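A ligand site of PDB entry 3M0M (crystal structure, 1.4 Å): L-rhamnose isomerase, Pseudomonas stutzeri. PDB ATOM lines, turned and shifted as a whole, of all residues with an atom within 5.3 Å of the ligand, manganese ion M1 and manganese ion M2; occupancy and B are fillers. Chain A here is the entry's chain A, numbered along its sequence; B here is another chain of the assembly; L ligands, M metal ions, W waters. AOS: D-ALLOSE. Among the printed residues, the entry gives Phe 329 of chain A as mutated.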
ATOM      1  N   TRP A  57       2.212 -14.235  38.462  1.00  0.00           N
ATOM      2  CA  TRP A  57       1.761 -15.486  37.871  1.00  0.00           C
ATOM      3  C   TRP A  57       2.902 -16.417  37.446  1.00  0.00           C
ATOM      4  O   TRP A  57       2.659 -17.531  36.995  1.00  0.00           O
ATOM      5  CB  TRP A  57       0.843 -15.205  36.683  1.00  0.00           C
ATOM      6  CG  TRP A  57       1.478 -14.433  35.555  1.00  0.00           C
ATOM      7  CD1 TRP A  57       2.155 -14.955  34.486  1.00  0.00           C
ATOM      8  CD2 TRP A  57       1.493 -13.016  35.385  1.00  0.00           C
ATOM      9  NE1 TRP A  57       2.579 -13.939  33.656  1.00  0.00           N
ATOM     10  CE2 TRP A  57       2.178 -12.739  34.181  1.00  0.00           C
ATOM     11  CE3 TRP A  57       0.978 -11.940  36.135  1.00  0.00           C
ATOM     12  CZ2 TRP A  57       2.382 -11.434  33.704  1.00  0.00           C
ATOM     13  CZ3 TRP A  57       1.176 -10.643  35.661  1.00  0.00           C
ATOM     14  CH2 TRP A  57       1.871 -10.401  34.455  1.00  0.00           C
ATOM     15  N   HIS A 101      -1.872  -9.291  38.767  1.00  0.00           N
ATOM     16  CA  HIS A 101      -2.897  -9.645  37.801  1.00  0.00           C
ATOM     17  C   HIS A 101      -4.210  -9.778  38.574  1.00  0.00           C
ATOM     18  O   HIS A 101      -4.283 -10.510  39.557  1.00  0.00           O
ATOM     19  CB  HIS A 101      -2.542 -10.981  37.119  1.00  0.00           C
ATOM     20  CG  HIS A 101      -2.929 -11.043  35.671  1.00  0.00           C
ATOM     21  ND1 HIS A 101      -4.235 -10.960  35.241  1.00  0.00           N
ATOM     22  CD2 HIS A 101      -2.175 -11.176  34.564  1.00  0.00           C
ATOM     23  CE1 HIS A 101      -4.268 -11.028  33.921  1.00  0.00           C
ATOM     24  NE2 HIS A 101      -3.030 -11.163  33.486  1.00  0.00           N
ATOM     25  N   TRP A 104      -6.758 -12.578  39.907  1.00  0.00           N
ATOM     26  CA  TRP A 104      -5.906 -13.598  40.529  1.00  0.00           C
ATOM     27  C   TRP A 104      -5.315 -13.124  41.845  1.00  0.00           C
ATOM     28  O   TRP A 104      -5.335 -13.837  42.847  1.00  0.00           O
ATOM     29  CB  TRP A 104      -4.758 -14.025  39.605  1.00  0.00           C
ATOM     30  CG  TRP A 104      -5.173 -14.709  38.333  1.00  0.00           C
ATOM     31  CD1 TRP A 104      -6.368 -15.307  38.064  1.00  0.00           C
ATOM     32  CD2 TRP A 104      -4.370 -14.853  37.160  1.00  0.00           C
ATOM     33  NE1 TRP A 104      -6.361 -15.825  36.790  1.00  0.00           N
ATOM     34  CE2 TRP A 104      -5.151 -15.562  36.208  1.00  0.00           C
ATOM     35  CE3 TRP A 104      -3.070 -14.468  36.815  1.00  0.00           C
ATOM     36  CZ2 TRP A 104      -4.661 -15.880  34.934  1.00  0.00           C
ATOM     37  CZ3 TRP A 104      -2.587 -14.780  35.544  1.00  0.00           C
ATOM     38  CH2 TRP A 104      -3.392 -15.482  34.624  1.00  0.00           C
ATOM     39  N   ASN A 127      -2.395  -5.654  35.645  1.00  0.00           N
ATOM     40  CA  ASN A 127      -2.849  -6.437  34.508  1.00  0.00           C
ATOM     41  C   ASN A 127      -4.298  -6.846  34.745  1.00  0.00           C
ATOM     42  O   ASN A 127      -4.604  -7.448  35.769  1.00  0.00           O
ATOM     43  CB  ASN A 127      -2.000  -7.700  34.346  1.00  0.00           C
ATOM     44  CG  ASN A 127      -0.554  -7.394  34.017  1.00  0.00           C
ATOM     45  OD1 ASN A 127      -0.170  -7.263  32.859  1.00  0.00           O
ATOM     46  ND2 ASN A 127       0.266  -7.262  35.057  1.00  0.00           N
ATOM     47  N   SER A 128      -5.171  -6.496  33.806  1.00  0.00           N
ATOM     48  CA  SER A 128      -6.589  -6.835  33.916  1.00  0.00           C
ATOM     49  C   SER A 128      -6.830  -8.223  33.317  1.00  0.00           C
ATOM     50  O   SER A 128      -6.019  -8.725  32.549  1.00  0.00           O
ATOM     51  CB  SER A 128      -7.444  -5.803  33.185  1.00  0.00           C
ATOM     52  OG  SER A 128      -7.021  -5.660  31.844  1.00  0.00           O
ATOM     53  N   PHE A 131     -10.338 -12.396  30.047  1.00  0.00           N
ATOM     54  CA  PHE A 131     -10.149 -13.513  29.139  1.00  0.00           C
ATOM     55  C   PHE A 131     -10.597 -14.805  29.835  1.00  0.00           C
ATOM     56  O   PHE A 131     -10.349 -15.912  29.349  1.00  0.00           O
ATOM     57  CB  PHE A 131      -8.684 -13.620  28.677  1.00  0.00           C
ATOM     58  CG  PHE A 131      -7.673 -13.639  29.806  1.00  0.00           C
ATOM     59  CD1 PHE A 131      -7.454 -14.785  30.555  1.00  0.00           C
ATOM     60  CD2 PHE A 131      -6.929 -12.498  30.098  1.00  0.00           C
ATOM     61  CE1 PHE A 131      -6.503 -14.805  31.569  1.00  0.00           C
ATOM     62  CE2 PHE A 131      -5.979 -12.505  31.111  1.00  0.00           C
ATOM     63  CZ  PHE A 131      -5.771 -13.658  31.854  1.00  0.00           C
ATOM     64  N   TRP A 179      -4.482  -7.044  28.002  1.00  0.00           N
ATOM     65  CA  TRP A 179      -4.354  -8.118  27.019  1.00  0.00           C
ATOM     66  C   TRP A 179      -5.648  -8.886  27.124  1.00  0.00           C
ATOM     67  O   TRP A 179      -6.063  -9.284  28.216  1.00  0.00           O
ATOM     68  CB  TRP A 179      -3.203  -9.078  27.316  1.00  0.00           C
ATOM     69  CG  TRP A 179      -3.256 -10.260  26.378  1.00  0.00           C
ATOM     70  CD1 TRP A 179      -2.937 -10.261  25.038  1.00  0.00           C
ATOM     71  CD2 TRP A 179      -3.788 -11.564  26.662  1.00  0.00           C
ATOM     72  NE1 TRP A 179      -3.251 -11.470  24.482  1.00  0.00           N
ATOM     73  CE2 TRP A 179      -3.767 -12.292  25.450  1.00  0.00           C
ATOM     74  CE3 TRP A 179      -4.271 -12.180  27.809  1.00  0.00           C
ATOM     75  CZ2 TRP A 179      -4.225 -13.622  25.362  1.00  0.00           C
ATOM     76  CZ3 TRP A 179      -4.732 -13.502  27.733  1.00  0.00           C
ATOM     77  CH2 TRP A 179      -4.704 -14.202  26.506  1.00  0.00           C
ATOM     78  N   GLU A 219      -1.618  -4.869  24.616  1.00  0.00           N
ATOM     79  CA  GLU A 219      -0.711  -5.942  24.217  1.00  0.00           C
ATOM     80  C   GLU A 219      -1.256  -6.784  23.059  1.00  0.00           C
ATOM     81  O   GLU A 219      -2.272  -7.454  23.209  1.00  0.00           O
ATOM     82  CB  GLU A 219      -0.435  -6.835  25.428  1.00  0.00           C
ATOM     83  CG  GLU A 219       0.548  -7.967  25.186  1.00  0.00           C
ATOM     84  CD  GLU A 219       0.771  -8.807  26.428  1.00  0.00           C
ATOM     85  OE1 GLU A 219       0.122  -8.560  27.460  1.00  0.00           O
ATOM     86  OE2 GLU A 219       1.609  -9.727  26.368  1.00  0.00           O
ATOM     87  N   LYS A 221      -1.289  -9.831  20.110  1.00  0.00           N
ATOM     88  CA  LYS A 221      -0.968 -11.259  20.075  1.00  0.00           C
ATOM     89  C   LYS A 221      -1.575 -11.847  18.806  1.00  0.00           C
ATOM     90  O   LYS A 221      -2.760 -11.677  18.556  1.00  0.00           O
ATOM     91  CB  LYS A 221      -1.537 -11.958  21.310  1.00  0.00           C
ATOM     92  CG  LYS A 221      -1.009 -13.368  21.478  1.00  0.00           C
ATOM     93  CD  LYS A 221      -1.593 -14.040  22.719  1.00  0.00           C
ATOM     94  CE  LYS A 221      -0.914 -15.378  22.956  1.00  0.00           C
ATOM     95  NZ  LYS A 221      -1.488 -16.093  24.141  1.00  0.00           N
ATOM     96  N   GLU A 224      -4.241 -17.340  19.948  1.00  0.00           N
ATOM     97  CA  GLU A 224      -4.376 -18.012  21.252  1.00  0.00           C
ATOM     98  C   GLU A 224      -4.814 -17.014  22.312  1.00  0.00           C
ATOM     99  O   GLU A 224      -4.057 -16.125  22.692  1.00  0.00           O
ATOM    100  CB  GLU A 224      -3.077 -18.678  21.703  1.00  0.00           C
ATOM    101  CG  GLU A 224      -3.307 -19.551  22.953  1.00  0.00           C
ATOM    102  CD  GLU A 224      -2.037 -19.919  23.716  1.00  0.00           C
ATOM    103  OE1 GLU A 224      -1.061 -19.150  23.665  1.00  0.00           O
ATOM    104  OE2 GLU A 224      -2.048 -20.974  24.386  1.00  0.00           O
ATOM    105  N   LEU A 252       2.566  -2.529  24.151  1.00  0.00           N
ATOM    106  CA  LEU A 252       3.433  -3.439  24.879  1.00  0.00           C
ATOM    107  C   LEU A 252       3.768  -4.599  23.941  1.00  0.00           C
ATOM    108  O   LEU A 252       2.870  -5.188  23.319  1.00  0.00           O
ATOM    109  CB  LEU A 252       2.740  -3.949  26.147  1.00  0.00           C
ATOM    110  CG  LEU A 252       3.631  -4.809  27.036  1.00  0.00           C
ATOM    111  CD1 LEU A 252       3.440  -4.430  28.501  1.00  0.00           C
ATOM    112  CD2 LEU A 252       3.327  -6.278  26.801  1.00  0.00           C
ATOM    113  N   ASP A 254       5.247  -8.290  23.565  1.00  0.00           N
ATOM    114  CA  ASP A 254       5.560  -9.550  24.246  1.00  0.00           C
ATOM    115  C   ASP A 254       6.310 -10.350  23.186  1.00  0.00           C
ATOM    116  O   ASP A 254       5.759 -10.656  22.125  1.00  0.00           O
ATOM    117  CB  ASP A 254       4.271 -10.258  24.664  1.00  0.00           C
ATOM    118  CG  ASP A 254       4.532 -11.541  25.447  1.00  0.00           C
ATOM    119  OD1 ASP A 254       5.332 -12.370  24.959  1.00  0.00           O
ATOM    120  OD2 ASP A 254       3.943 -11.727  26.536  1.00  0.00           O
ATOM    121  N   HIS A 257       4.652 -13.238  21.008  1.00  0.00           N
ATOM    122  CA  HIS A 257       3.345 -12.976  20.401  1.00  0.00           C
ATOM    123  C   HIS A 257       3.363 -12.654  18.900  1.00  0.00           C
ATOM    124  O   HIS A 257       2.401 -12.059  18.390  1.00  0.00           O
ATOM    125  CB  HIS A 257       2.665 -11.816  21.143  1.00  0.00           C
ATOM    126  CG  HIS A 257       2.186 -12.184  22.513  1.00  0.00           C
ATOM    127  ND1 HIS A 257       1.306 -11.391  23.215  1.00  0.00           N
ATOM    128  CD2 HIS A 257       2.438 -13.261  23.297  1.00  0.00           C
ATOM    129  CE1 HIS A 257       1.030 -11.973  24.378  1.00  0.00           C
ATOM    130  NE2 HIS A 257       1.710 -13.103  24.447  1.00  0.00           N
ATOM    131  N   HIS A 281       7.359  -7.522  27.430  1.00  0.00           N
ATOM    132  CA  HIS A 281       7.049  -8.722  28.189  1.00  0.00           C
ATOM    133  C   HIS A 281       8.113  -9.678  27.657  1.00  0.00           C
ATOM    134  O   HIS A 281       8.059 -10.113  26.503  1.00  0.00           O
ATOM    135  CB  HIS A 281       5.638  -9.256  27.902  1.00  0.00           C
ATOM    136  CG  HIS A 281       4.599  -8.727  28.825  1.00  0.00           C
ATOM    137  ND1 HIS A 281       3.328  -9.245  28.903  1.00  0.00           N
ATOM    138  CD2 HIS A 281       4.640  -7.711  29.726  1.00  0.00           C
ATOM    139  CE1 HIS A 281       2.623  -8.574  29.799  1.00  0.00           C
ATOM    140  NE2 HIS A 281       3.401  -7.643  30.319  1.00  0.00           N
ATOM    141  N   ASP A 289       3.576 -19.004  21.523  1.00  0.00           N
ATOM    142  CA  ASP A 289       3.755 -18.173  22.714  1.00  0.00           C
ATOM    143  C   ASP A 289       4.118 -19.138  23.848  1.00  0.00           C
ATOM    144  O   ASP A 289       3.379 -19.299  24.816  1.00  0.00           O
ATOM    145  CB  ASP A 289       2.479 -17.406  23.036  1.00  0.00           C
ATOM    146  CG  ASP A 289       2.638 -16.491  24.230  1.00  0.00           C
ATOM    147  OD1 ASP A 289       3.773 -16.013  24.447  1.00  0.00           O
ATOM    148  OD2 ASP A 289       1.629 -16.251  24.930  1.00  0.00           O
ATOM    149  N   ASP A 291       6.240 -19.021  26.249  1.00  0.00           N
ATOM    150  CA  ASP A 291       6.490 -18.443  27.568  1.00  0.00           C
ATOM    151  C   ASP A 291       7.632 -19.063  28.351  1.00  0.00           C
ATOM    152  O   ASP A 291       7.568 -19.212  29.575  1.00  0.00           O
ATOM    153  CB  ASP A 291       5.208 -18.479  28.408  1.00  0.00           C
ATOM    154  CG  ASP A 291       4.215 -17.416  27.979  1.00  0.00           C
ATOM    155  OD1 ASP A 291       4.673 -16.288  27.707  1.00  0.00           O
ATOM    156  OD2 ASP A 291       3.005 -17.690  27.925  1.00  0.00           O
ATOM    157  N   ASP A 327       7.280 -12.041  31.442  1.00  0.00           N
ATOM    158  CA  ASP A 327       5.980 -12.701  31.345  1.00  0.00           C
ATOM    159  C   ASP A 327       6.293 -14.112  30.917  1.00  0.00           C
ATOM    160  O   ASP A 327       6.491 -14.383  29.727  1.00  0.00           O
ATOM    161  CB  ASP A 327       5.065 -12.039  30.315  1.00  0.00           C
ATOM    162  CG  ASP A 327       3.705 -12.725  30.236  1.00  0.00           C
ATOM    163  OD1 ASP A 327       3.482 -13.683  31.005  1.00  0.00           O
ATOM    164  OD2 ASP A 327       2.865 -12.298  29.419  1.00  0.00           O
ATOM    165  N   PHE A 329       5.871 -18.600  32.083  1.00  0.00           N
ATOM    166  CA  PHE A 329       5.216 -19.653  32.844  1.00  0.00           C
ATOM    167  C   PHE A 329       6.262 -20.742  32.955  1.00  0.00           C
ATOM    168  O   PHE A 329       6.967 -21.032  31.989  1.00  0.00           O
ATOM    169  CB  PHE A 329       3.956 -20.171  32.137  1.00  0.00           C
ATOM    170  CG  PHE A 329       2.776 -19.258  32.285  1.00  0.00           C
ATOM    171  CD1 PHE A 329       2.417 -18.381  31.266  1.00  0.00           C
ATOM    172  CD2 PHE A 329       2.053 -19.233  33.475  1.00  0.00           C
ATOM    173  CE1 PHE A 329       1.345 -17.494  31.422  1.00  0.00           C
ATOM    174  CE2 PHE A 329       0.988 -18.345  33.649  1.00  0.00           C
ATOM    175  CZ  PHE A 329       0.638 -17.468  32.615  1.00  0.00           C
ATOM    176  N   ARG B  65      -5.441 -22.969  27.514  1.00  0.00           N
ATOM    177  CA  ARG B  65      -4.774 -22.880  28.812  1.00  0.00           C
ATOM    178  C   ARG B  65      -5.249 -21.651  29.588  1.00  0.00           C
ATOM    179  O   ARG B  65      -5.037 -21.555  30.793  1.00  0.00           O
ATOM    180  CB  ARG B  65      -3.254 -22.825  28.654  1.00  0.00           C
ATOM    181  CG  ARG B  65      -2.743 -21.643  27.872  1.00  0.00           C
ATOM    182  CD  ARG B  65      -1.213 -21.552  27.916  1.00  0.00           C
ATOM    183  NE  ARG B  65      -0.737 -20.607  26.913  1.00  0.00           N
ATOM    184  CZ  ARG B  65       0.278 -19.765  27.082  1.00  0.00           C
ATOM    185  NH1 ARG B  65       0.963 -19.727  28.222  1.00  0.00           N
ATOM    186  NH2 ARG B  65       0.608 -18.938  26.098  1.00  0.00           N
ATOM    187  N   PHE B  66      -5.919 -20.729  28.903  1.00  0.00           N
ATOM    188  CA  PHE B  66      -6.423 -19.514  29.528  1.00  0.00           C
ATOM    189  C   PHE B  66      -7.807 -19.644  30.146  1.00  0.00           C
ATOM    190  O   PHE B  66      -8.094 -19.037  31.177  1.00  0.00           O
ATOM    191  CB  PHE B  66      -6.426 -18.364  28.518  1.00  0.00           C
ATOM    192  CG  PHE B  66      -5.048 -17.931  28.112  1.00  0.00           C
ATOM    193  CD1 PHE B  66      -4.248 -17.202  28.989  1.00  0.00           C
ATOM    194  CD2 PHE B  66      -4.526 -18.294  26.882  1.00  0.00           C
ATOM    195  CE1 PHE B  66      -2.952 -16.852  28.647  1.00  0.00           C
ATOM    196  CE2 PHE B  66      -3.227 -17.952  26.529  1.00  0.00           C
ATOM    197  CZ  PHE B  66      -2.433 -17.231  27.409  1.00  0.00           C
HETATM  198  C1  AOS L   1      -1.153 -13.578  27.134  1.00  0.00           C
HETATM  199  O1  AOS L   1      -0.847 -14.351  26.216  1.00  0.00           O
HETATM  200  C2  AOS L   1      -0.280 -12.363  27.396  1.00  0.00           C
HETATM  201  O2  AOS L   1       1.076 -12.748  27.506  1.00  0.00           O
HETATM  202  C3  AOS L   1      -0.733 -11.559  28.630  1.00  0.00           C
HETATM  203  O3  AOS L   1       0.336 -10.726  29.071  1.00  0.00           O
HETATM  204  C4  AOS L   1      -1.279 -12.378  29.809  1.00  0.00           C
HETATM  205  O4  AOS L   1      -2.064 -11.517  30.629  1.00  0.00           O
HETATM  206  C5  AOS L   1      -0.162 -12.992  30.657  1.00  0.00           C
HETATM  207  O5  AOS L   1       0.648 -13.850  29.859  1.00  0.00           O
HETATM  208  C6  AOS L   1      -0.769 -13.789  31.807  1.00  0.00           C
HETATM  209  O6  AOS L   1      -1.522 -14.880  31.297  1.00  0.00           O
HETATM  210 MN    MN M   1       2.391 -11.006  27.907  1.00  0.00          MN
HETATM  211 MN    MN M   2       1.331 -14.455  26.093  1.00  0.00          MN
HETATM  212  O   HOH W   1      -1.551  -8.711  30.766  1.00  0.00           O
HETATM  213  O   HOH W   2       3.298 -14.601  26.440  1.00  0.00           O
HETATM  214  O   HOH W   3       1.173 -15.614  27.846  1.00  0.00           O
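NZ of Lys 221 lies close to O1 of the ligand (2.8 Å).
An oxygen (O4) of the ligand sits at hydrogen-bond distance from a ring nitrogen (NE2) of His 101, at 3.0 Å.
The backbone carbonyl oxygen of Asp 289 lies within hydrogen-bond range of the guanidinium group of Arg 65 of chain B (3.1 Å).
The side-chain carboxylate (OD1) of Asp 327 lies within hydrogen-bond range of the indole nitrogen (NE1) of Trp 57.
The side-chain carboxylate (OE1) of Glu 224 lies within salt-bridge range of the side-chain amino group (NZ) of Lys 221 (3.1 Å).
The side-chain carboxylate of Asp 289 sits close to the side-chain amino group of Lys 221, 3.2 Å away.
N of Phe 329 sits at hydrogen-bond distance from O of Asp 291 (3.1 Å).
Trp 57 touches the ligand.
CH2 of Trp 104 touches O6 of the ligand, at 3.9 Å.
Trp 179 touches the ligand.
CZ of Phe 329 touches O6 of the ligand, at 3.6 Å.
Phe 66 of chain B touches the ligand (CZ to O1, 3.5 Å).
Hydrophobic or aromatic side chains that line the ligand: Trp 57, His 101, Trp 104, Trp 179, His 257, His 281, Phe 329 and Phe 66 of chain B.
Within 4 Å of the ligand: Trp 57, His 101, Trp 104, Trp 179, Glu 219, Lys 221, Asp 254, His 257, His 281, Asp 289, Asp 327, Phe 329 and Phe 66 of chain B.
Of the 20 residues printed, 5 come within 4 Å of manganese ion M1.
Residues that only touch manganese ion M2: Lys 221.
Within 4 Å of manganese ion M2: Lys 221, Asp 254, His 257 and Asp 289.
Manganese ion M1 is bound by the side-chain carboxylate (OD2) of Asp 327, 2.0 Å away.
Manganese ion M1 is bound by the side-chain carboxylate (OE2) of Glu 219.
The side-chain carboxylate (OD2) of Asp 254 is bound to manganese ion M1 (2.2 Å).
O2 of the ligand is bound to manganese ion M1 (2.2 Å).
ND1 of His 281 is bound to manganese ion M1 (2.2 Å).
An oxygen (O3) of the ligand binds manganese ion M1, 2.4 Å away.
Manganese ion M1 has six donor atoms within binding distance.
Manganese ion M2 is bound by water W2 (2.0 Å), water W3 (2.1 Å), the side-chain carboxylate (OD2) of Asp 289 (2.2 Å), a ring nitrogen (NE2) of His 257 (2.2 Å), an oxygen (O1) of the ligand (2.2 Å) and an oxygen (O2) of the ligand (2.2 Å).
Water W3 lies within hydrogen-bond range of O5 of the ligand (2.7 Å) and OD2 of Asp 291 (2.8 Å).
Water W1 bridges O4 of the ligand (2.9 Å) and OD1 of Asn 127 (2.9 Å).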
